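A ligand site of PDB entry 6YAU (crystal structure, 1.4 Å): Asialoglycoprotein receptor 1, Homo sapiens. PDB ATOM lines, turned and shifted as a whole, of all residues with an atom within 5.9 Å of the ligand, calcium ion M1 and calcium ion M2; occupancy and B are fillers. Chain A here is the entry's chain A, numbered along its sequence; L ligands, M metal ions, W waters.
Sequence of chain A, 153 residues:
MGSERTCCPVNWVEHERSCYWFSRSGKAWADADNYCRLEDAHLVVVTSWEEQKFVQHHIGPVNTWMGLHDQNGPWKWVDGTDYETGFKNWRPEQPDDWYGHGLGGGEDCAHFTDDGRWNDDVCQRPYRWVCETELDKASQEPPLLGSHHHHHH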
ATOM      1  N   ASN A  63      26.450  13.767  18.011  1.00  0.00           N
ATOM      2  CA  ASN A  63      25.013  14.088  18.006  1.00  0.00           C
ATOM      3  C   ASN A  63      24.693  14.780  16.695  1.00  0.00           C
ATOM      4  O   ASN A  63      25.326  15.781  16.385  1.00  0.00           O
ATOM      5  CB  ASN A  63      24.637  14.981  19.176  1.00  0.00           C
ATOM      6  CG  ASN A  63      24.620  14.229  20.468  1.00  0.00           C
ATOM      7  OD1 ASN A  63      25.035  14.728  21.524  1.00  0.00           O
ATOM      8  ND2 ASN A  63      24.088  13.026  20.409  1.00  0.00           N
ATOM      9  N   ASP A  70       8.365  15.984  16.110  1.00  0.00           N
ATOM     10  CA  ASP A  70       6.975  15.992  16.583  1.00  0.00           C
ATOM     11  C   ASP A  70       6.563  17.373  17.118  1.00  0.00           C
ATOM     12  O   ASP A  70       5.807  17.452  18.069  1.00  0.00           O
ATOM     13  CB  ASP A  70       6.680  14.852  17.588  1.00  0.00           C
ATOM     14  CG  ASP A  70       7.181  15.073  19.002  1.00  0.00           C
ATOM     15  OD1 ASP A  70       8.088  15.888  19.191  1.00  0.00           O
ATOM     16  OD2 ASP A  70       6.667  14.407  19.933  1.00  0.00           O
ATOM     17  N   TRP A  75       4.846  12.249  15.649  1.00  0.00           N
ATOM     18  CA  TRP A  75       6.148  12.118  14.996  1.00  0.00           C
ATOM     19  C   TRP A  75       5.971  11.982  13.504  1.00  0.00           C
ATOM     20  O   TRP A  75       5.134  11.188  13.056  1.00  0.00           O
ATOM     21  CB  TRP A  75       6.925  10.914  15.550  1.00  0.00           C
ATOM     22  CG  TRP A  75       7.526  11.183  16.899  1.00  0.00           C
ATOM     23  CD1 TRP A  75       7.019  10.831  18.120  1.00  0.00           C
ATOM     24  CD2 TRP A  75       8.721  11.910  17.157  1.00  0.00           C
ATOM     25  NE1 TRP A  75       7.819  11.314  19.125  1.00  0.00           N
ATOM     26  CE2 TRP A  75       8.876  12.007  18.552  1.00  0.00           C
ATOM     27  CE3 TRP A  75       9.671  12.549  16.327  1.00  0.00           C
ATOM     28  CZ2 TRP A  75       9.977  12.635  19.146  1.00  0.00           C
ATOM     29  CZ3 TRP A  75      10.752  13.191  16.917  1.00  0.00           C
ATOM     30  CH2 TRP A  75      10.869  13.274  18.306  1.00  0.00           C
ATOM     31  N   ARG A  91      16.886   4.852  21.103  1.00  0.00           N
ATOM     32  CA  ARG A  91      17.579   4.260  22.235  1.00  0.00           C
ATOM     33  C   ARG A  91      16.451   3.796  23.172  1.00  0.00           C
ATOM     34  O   ARG A  91      15.457   4.522  23.308  1.00  0.00           O
ATOM     35  CB  ARG A  91      18.446   5.291  22.970  1.00  0.00           C
ATOM     36  CG  ARG A  91      19.206   4.685  24.174  1.00  0.00           C
ATOM     37  CD  ARG A  91      20.248   5.601  24.738  1.00  0.00           C
ATOM     38  NE  ARG A  91      19.656   6.759  25.393  1.00  0.00           N
ATOM     39  CZ  ARG A  91      20.039   8.015  25.198  1.00  0.00           C
ATOM     40  NH1 ARG A  91      21.023   8.293  24.348  1.00  0.00           N
ATOM     41  NH2 ARG A  91      19.458   9.002  25.866  1.00  0.00           N
ATOM     42  N   GLN A  94      13.437   5.902  24.760  1.00  0.00           N
ATOM     43  CA  GLN A  94      13.244   7.110  23.970  1.00  0.00           C
ATOM     44  C   GLN A  94      12.201   6.758  22.900  1.00  0.00           C
ATOM     45  O   GLN A  94      12.081   5.574  22.542  1.00  0.00           O
ATOM     46  CB  GLN A  94      14.563   7.605  23.338  1.00  0.00           C
ATOM     47  CG  GLN A  94      15.686   7.865  24.349  1.00  0.00           C
ATOM     48  CD  GLN A  94      15.471   9.035  25.307  1.00  0.00           C
ATOM     49  OE1 GLN A  94      14.649   9.944  25.083  1.00  0.00           O
ATOM     50  NE2 GLN A  94      16.228   9.031  26.403  1.00  0.00           N
ATOM     51  N   PRO A  95      11.436   7.730  22.372  1.00  0.00           N
ATOM     52  CA  PRO A  95      11.428   9.161  22.734  1.00  0.00           C
ATOM     53  C   PRO A  95      10.734   9.402  24.080  1.00  0.00           C
ATOM     54  O   PRO A  95       9.775   8.725  24.370  1.00  0.00           O
ATOM     55  CB  PRO A  95      10.658   9.803  21.578  1.00  0.00           C
ATOM     56  CG  PRO A  95       9.729   8.738  21.066  1.00  0.00           C
ATOM     57  CD  PRO A  95      10.376   7.402  21.391  1.00  0.00           C
ATOM     58  N   ASP A  96      11.229  10.332  24.907  1.00  0.00           N
ATOM     59  CA  ASP A  96      10.601  10.562  26.211  1.00  0.00           C
ATOM     60  C   ASP A  96       9.979  11.964  26.364  1.00  0.00           C
ATOM     61  O   ASP A  96       9.377  12.232  27.392  1.00  0.00           O
ATOM     62  CB  ASP A  96      11.589  10.273  27.354  1.00  0.00           C
ATOM     63  CG  ASP A  96      12.832  11.136  27.332  1.00  0.00           C
ATOM     64  OD1 ASP A  96      12.975  11.928  26.401  1.00  0.00           O
ATOM     65  OD2 ASP A  96      13.657  11.021  28.251  1.00  0.00           O
ATOM     66  N   ASP A  97      10.127  12.846  25.366  1.00  0.00           N
ATOM     67  CA  ASP A  97       9.580  14.224  25.439  1.00  0.00           C
ATOM     68  C   ASP A  97       9.966  14.884  26.768  1.00  0.00           C
ATOM     69  O   ASP A  97       9.121  15.514  27.409  1.00  0.00           O
ATOM     70  CB  ASP A  97       8.037  14.220  25.299  1.00  0.00           C
ATOM     71  CG  ASP A  97       7.458  15.559  24.898  1.00  0.00           C
ATOM     72  OD1 ASP A  97       8.025  16.214  23.983  1.00  0.00           O
ATOM     73  OD2 ASP A  97       6.419  15.952  25.502  1.00  0.00           O
ATOM     74  N   TRP A  98      11.228  14.731  27.172  1.00  0.00           N
ATOM     75  CA  TRP A  98      11.732  15.217  28.470  1.00  0.00           C
ATOM     76  C   TRP A  98      11.567  16.715  28.716  1.00  0.00           C
ATOM     77  O   TRP A  98      11.880  17.536  27.834  1.00  0.00           O
ATOM     78  CB  TRP A  98      13.188  14.804  28.641  1.00  0.00           C
ATOM     79  CG  TRP A  98      13.795  14.948  30.009  1.00  0.00           C
ATOM     80  CD1 TRP A  98      13.297  14.466  31.191  1.00  0.00           C
ATOM     81  CD2 TRP A  98      15.111  15.439  30.313  1.00  0.00           C
ATOM     82  NE1 TRP A  98      14.189  14.683  32.212  1.00  0.00           N
ATOM     83  CE2 TRP A  98      15.336  15.247  31.694  1.00  0.00           C
ATOM     84  CE3 TRP A  98      16.103  16.085  29.545  1.00  0.00           C
ATOM     85  CZ2 TRP A  98      16.503  15.690  32.332  1.00  0.00           C
ATOM     86  CZ3 TRP A  98      17.294  16.470  30.166  1.00  0.00           C
ATOM     87  CH2 TRP A  98      17.488  16.252  31.540  1.00  0.00           C
ATOM     88  N   GLY A 106       9.042  20.272  25.902  1.00  0.00           N
ATOM     89  CA  GLY A 106       9.514  18.901  25.957  1.00  0.00           C
ATOM     90  C   GLY A 106      10.713  18.767  25.053  1.00  0.00           C
ATOM     91  O   GLY A 106      11.636  19.578  25.126  1.00  0.00           O
ATOM     92  N   GLU A 107      10.681  17.752  24.174  1.00  0.00           N
ATOM     93  CA  GLU A 107      11.762  17.487  23.219  1.00  0.00           C
ATOM     94  C   GLU A 107      11.091  17.082  21.929  1.00  0.00           C
ATOM     95  O   GLU A 107      10.342  16.122  21.882  1.00  0.00           O
ATOM     96  CB  GLU A 107      12.687  16.386  23.755  1.00  0.00           C
ATOM     97  CG  GLU A 107      13.564  16.819  24.934  1.00  0.00           C
ATOM     98  CD  GLU A 107      14.454  15.719  25.479  1.00  0.00           C
ATOM     99  OE1 GLU A 107      15.600  16.005  25.884  1.00  0.00           O
ATOM    100  OE2 GLU A 107      14.006  14.551  25.469  1.00  0.00           O
ATOM    101  N   ASP A 108      11.321  17.831  20.872  1.00  0.00           N
ATOM    102  CA  ASP A 108      10.552  17.586  19.667  1.00  0.00           C
ATOM    103  C   ASP A 108      11.364  17.265  18.431  1.00  0.00           C
ATOM    104  O   ASP A 108      10.764  17.088  17.373  1.00  0.00           O
ATOM    105  CB  ASP A 108       9.646  18.806  19.388  1.00  0.00           C
ATOM    106  CG  ASP A 108       8.581  19.063  20.441  1.00  0.00           C
ATOM    107  OD1 ASP A 108       8.270  18.125  21.237  1.00  0.00           O
ATOM    108  OD2 ASP A 108       8.069  20.191  20.487  1.00  0.00           O
ATOM    109  N   HIS A 111      17.609  13.067  16.850  1.00  0.00           N
ATOM    110  CA  HIS A 111      19.003  13.070  16.422  1.00  0.00           C
ATOM    111  C   HIS A 111      19.634  11.705  16.623  1.00  0.00           C
ATOM    112  O   HIS A 111      19.152  10.894  17.433  1.00  0.00           O
ATOM    113  CB  HIS A 111      19.815  14.152  17.152  1.00  0.00           C
ATOM    114  CG  HIS A 111      19.971  13.920  18.619  1.00  0.00           C
ATOM    115  ND1 HIS A 111      21.171  13.482  19.191  1.00  0.00           N
ATOM    116  CD2 HIS A 111      19.075  14.131  19.618  1.00  0.00           C
ATOM    117  CE1 HIS A 111      20.947  13.414  20.492  1.00  0.00           C
ATOM    118  NE2 HIS A 111      19.706  13.776  20.800  1.00  0.00           N
ATOM    119  N   THR A 113      22.506   9.667  18.263  1.00  0.00           N
ATOM    120  CA  THR A 113      23.364   9.899  19.425  1.00  0.00           C
ATOM    121  C   THR A 113      24.754   9.352  19.019  1.00  0.00           C
ATOM    122  O   THR A 113      24.909   8.801  17.908  1.00  0.00           O
ATOM    123  CB  THR A 113      22.825   9.157  20.655  1.00  0.00           C
ATOM    124  OG1 THR A 113      22.866   7.748  20.379  1.00  0.00           O
ATOM    125  CG2 THR A 113      21.421   9.614  21.051  1.00  0.00           C
ATOM    126  N   ASN A 119      17.506   9.710  19.744  1.00  0.00           N
ATOM    127  CA  ASN A 119      16.978  10.390  20.927  1.00  0.00           C
ATOM    128  C   ASN A 119      16.198  11.617  20.468  1.00  0.00           C
ATOM    129  O   ASN A 119      16.527  12.222  19.429  1.00  0.00           O
ATOM    130  CB  ASN A 119      18.110  10.830  21.852  1.00  0.00           C
ATOM    131  CG  ASN A 119      17.622  11.677  23.032  1.00  0.00           C
ATOM    132  OD1 ASN A 119      16.742  11.268  23.794  1.00  0.00           O
ATOM    133  ND2 ASN A 119      18.144  12.875  23.177  1.00  0.00           N
ATOM    134  N   ASP A 120      15.113  11.912  21.178  1.00  0.00           N
ATOM    135  CA  ASP A 120      14.437  13.158  20.936  1.00  0.00           C
ATOM    136  C   ASP A 120      15.098  14.198  21.857  1.00  0.00           C
ATOM    137  O   ASP A 120      15.377  13.939  23.040  1.00  0.00           O
ATOM    138  CB  ASP A 120      12.909  13.069  21.191  1.00  0.00           C
ATOM    139  CG  ASP A 120      12.430  12.630  22.578  1.00  0.00           C
ATOM    140  OD1 ASP A 120      13.247  11.993  23.338  1.00  0.00           O
ATOM    141  OD2 ASP A 120      11.241  12.887  22.896  1.00  0.00           O
ATOM    142  N   ASP A 121      15.274  15.413  21.307  1.00  0.00           N
ATOM    143  CA  ASP A 121      15.923  16.454  22.087  1.00  0.00           C
ATOM    144  C   ASP A 121      15.346  17.827  21.790  1.00  0.00           C
ATOM    145  O   ASP A 121      14.490  17.991  20.915  1.00  0.00           O
ATOM    146  CB  ASP A 121      17.475  16.389  21.838  1.00  0.00           C
ATOM    147  CG  ASP A 121      18.376  16.820  23.015  1.00  0.00           C
ATOM    148  OD1 ASP A 121      19.533  16.305  23.108  1.00  0.00           O
ATOM    149  OD2 ASP A 121      17.927  17.646  23.825  1.00  0.00           O
ATOM    150  N   TYR A 127      23.401  21.068  16.836  1.00  0.00           N
ATOM    151  CA  TYR A 127      24.015  19.776  16.498  1.00  0.00           C
ATOM    152  C   TYR A 127      24.440  19.766  15.001  1.00  0.00           C
ATOM    153  O   TYR A 127      23.924  20.563  14.182  1.00  0.00           O
ATOM    154  CB  TYR A 127      23.022  18.617  16.692  1.00  0.00           C
ATOM    155  CG  TYR A 127      22.706  18.219  18.129  1.00  0.00           C
ATOM    156  CD1 TYR A 127      23.670  18.317  19.130  1.00  0.00           C
ATOM    157  CD2 TYR A 127      21.488  17.620  18.455  1.00  0.00           C
ATOM    158  CE1 TYR A 127      23.400  17.903  20.433  1.00  0.00           C
ATOM    159  CE2 TYR A 127      21.212  17.195  19.750  1.00  0.00           C
ATOM    160  CZ  TYR A 127      22.178  17.330  20.741  1.00  0.00           C
ATOM    161  OH  TYR A 127      21.943  16.877  22.008  1.00  0.00           O
HETATM  162  C1  LIG L   1      23.988  13.619  27.611  1.00  0.00           C
HETATM  163  C2  LIG L   1      23.712  12.524  28.620  1.00  0.00           C
HETATM  164  C3  LIG L   1      23.243  11.205  27.999  1.00  0.00           C
HETATM  165  C4  LIG L   1      22.365  10.369  28.919  1.00  0.00           C
HETATM  166  C5  LIG L   1      21.019  10.999  29.240  1.00  0.00           C
HETATM  167  C6  LIG L   1      17.146  12.551  29.160  1.00  0.00           C
HETATM  168  C7  LIG L   1      16.506  12.981  27.839  1.00  0.00           C
HETATM  169  C8  LIG L   1      17.561  13.584  26.912  1.00  0.00           C
HETATM  170  C9  LIG L   1      18.777  12.665  26.785  1.00  0.00           C
HETATM  171  N1  LIG L   1      23.422  14.795  27.867  1.00  0.00           N
HETATM  172  O1  LIG L   1      24.683  13.410  26.619  1.00  0.00           O
HETATM  173  O2  LIG L   1      20.328  11.281  28.018  1.00  0.00           O
HETATM  174  C10 LIG L   1      19.271  12.187  28.153  1.00  0.00           C
HETATM  175  O3  LIG L   1      18.214  11.608  28.891  1.00  0.00           O
HETATM  176  C11 LIG L   1      16.163  11.888  30.104  1.00  0.00           C
HETATM  177  O4  LIG L   1      16.754  11.636  31.380  1.00  0.00           O
HETATM  178  O5  LIG L   1      15.892  11.861  27.211  1.00  0.00           O
HETATM  179  O6  LIG L   1      17.006  13.777  25.625  1.00  0.00           O
HETATM  180  N2  LIG L   1      19.838  13.315  26.041  1.00  0.00           N
HETATM  181  C12 LIG L   1      20.631  12.695  25.161  1.00  0.00           C
HETATM  182  C13 LIG L   1      21.621  13.556  24.443  1.00  0.00           C
HETATM  183  O7  LIG L   1      20.528  11.483  24.928  1.00  0.00           O
HETATM  184 CA    CA M   1       7.849  15.680  21.597  1.00  0.00          CA
HETATM  185 CA    CA M   2      14.898  12.381  24.948  1.00  0.00          CA
HETATM  186  O   HOH W   1      21.267  15.276  29.834  1.00  0.00           O
HETATM  187  O   HOH W   2       5.736  14.717  22.613  1.00  0.00           O
HETATM  188  O   HOH W   3      22.329  17.505  26.634  1.00  0.00           O
HETATM  189  O   HOH W   4      18.316   8.889  28.557  1.00  0.00           O
HETATM  190  O   HOH W   5      23.100  10.403  24.125  1.00  0.00           O
HETATM  191  O   HOH W   6       8.745  13.646  22.187  1.00  0.00           O
HETATM  192  O   HOH W   7      20.054  16.268  25.854  1.00  0.00           O
HETATM  193  O   HOH W   8      25.171  15.148  24.427  1.00  0.00           O
HETATM  194  O   HOH W   9       5.729  17.066  21.399  1.00  0.00           O
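Calcium ion M1 is bound by water W6 (2.3 Å), the side-chain carboxylate (OD2) of Asp 70 (2.4 Å), the side-chain carboxylate (OD1) of Asp 70 (2.4 Å), the side-chain carboxylate (OD1) of Asp 97 (2.5 Å), the side-chain carboxylate (OD1) of Asp 108 (2.5 Å), water W2 (2.5 Å), water W9 (2.5 Å) and the backbone carbonyl oxygen (O) of Glu 107 (2.5 Å). Calcium ion M1 has eight donor atoms within binding distance.
CE3 of Trp 98 touches C7 of the ligand, at 3.6 Å. Asp 121 touches the ligand (OD1 to C13, 3.7 Å). Hydrophobic or aromatic side chains within 4 Å of the ligand: Trp 98. Of the 18 residues printed, 8 come within 4 Å of the ligand. The nearest printed residue that does not touch the ligand is His 111 (4.01 Å).
The guanidinium group (NH2) of Arg 91 sits at hydrogen-bond distance from an oxygen (O7) of the ligand, 2.9 Å away.
Of the 18 residues printed, 4 come within 4 Å of calcium ion M1. Along chain A the residues within 4 Å of calcium ion M1 span positions 70 to 108. The nearest printed residue that does not touch calcium ion M1 is Trp 75 (4.5 Å).
The side-chain carboxylate (OD1) of Asp 120 binds calcium ion M2 (2.3 Å). OE2 of Glu 107 binds calcium ion M2 (2.4 Å). OD1 of Asn 119 binds calcium ion M2, 2.4 Å away. OD1 of Asp 96 is bound to calcium ion M2 (2.5 Å). Calcium ion M2 is bound by OE1 of Gln 94 (2.5 Å). Calcium ion M2 is bound by the backbone carbonyl oxygen (O) of Asp 120 (2.5 Å). Calcium ion M2 is bound by O5 of the ligand, at 2.5 Å. Calcium ion M2 is bound by O6 of the ligand. Calcium ion M2 has eight donor atoms within binding distance.
The backbone NH of Asp 97 lies within hydrogen-bond range of the side-chain carboxylate of Asp 120, 2.7 Å away. N of Asp 108 lies within hydrogen-bond range of O of Asp 121 (3.2 Å). The indole nitrogen (NE1) of Trp 75 sits close to the side-chain carboxylate (OD2) of Asp 70 (3.4 Å). The side-chain carboxylate (OD1) of Asp 121 is in hydrogen-bond range of a ring nitrogen (NE2) of His 111, at 3.4 Å. OD1 of Asp 121 sits at hydrogen-bond distance from OH of Tyr 127 (2.7 Å). The side-chain carboxylate (OE2) of Glu 107 lies close to the backbone NH (N) of Trp 98 (3.3 Å). N of His 111 lies within hydrogen-bond range of O of Asn 119, at 2.9 Å. The side-chain amide nitrogen of Gln 94 sits close to the guanidinium group of Arg 91.
Water W4 lies within hydrogen-bond range of an oxygen (O3) of the ligand, the guanidinium group (NH2) of Arg 91 and the side-chain amide nitrogen (NE2) of Gln 94. Water W8 bridges an oxygen (O1) of the ligand (2.8 Å) and the side-chain amide oxygen of Asn 63 (2.9 Å). Water W5 bridges O7 of the ligand (2.9 Å) and NH1 of Arg 91 (3.0 Å). Water W7 bridges OD1 of Asp 121 (2.8 Å) and N2 of the ligand (3.0 Å).
Within 4 Å of calcium ion M2: Gln 94, Asp 96, Glu 107, Asn 119 and Asp 120.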
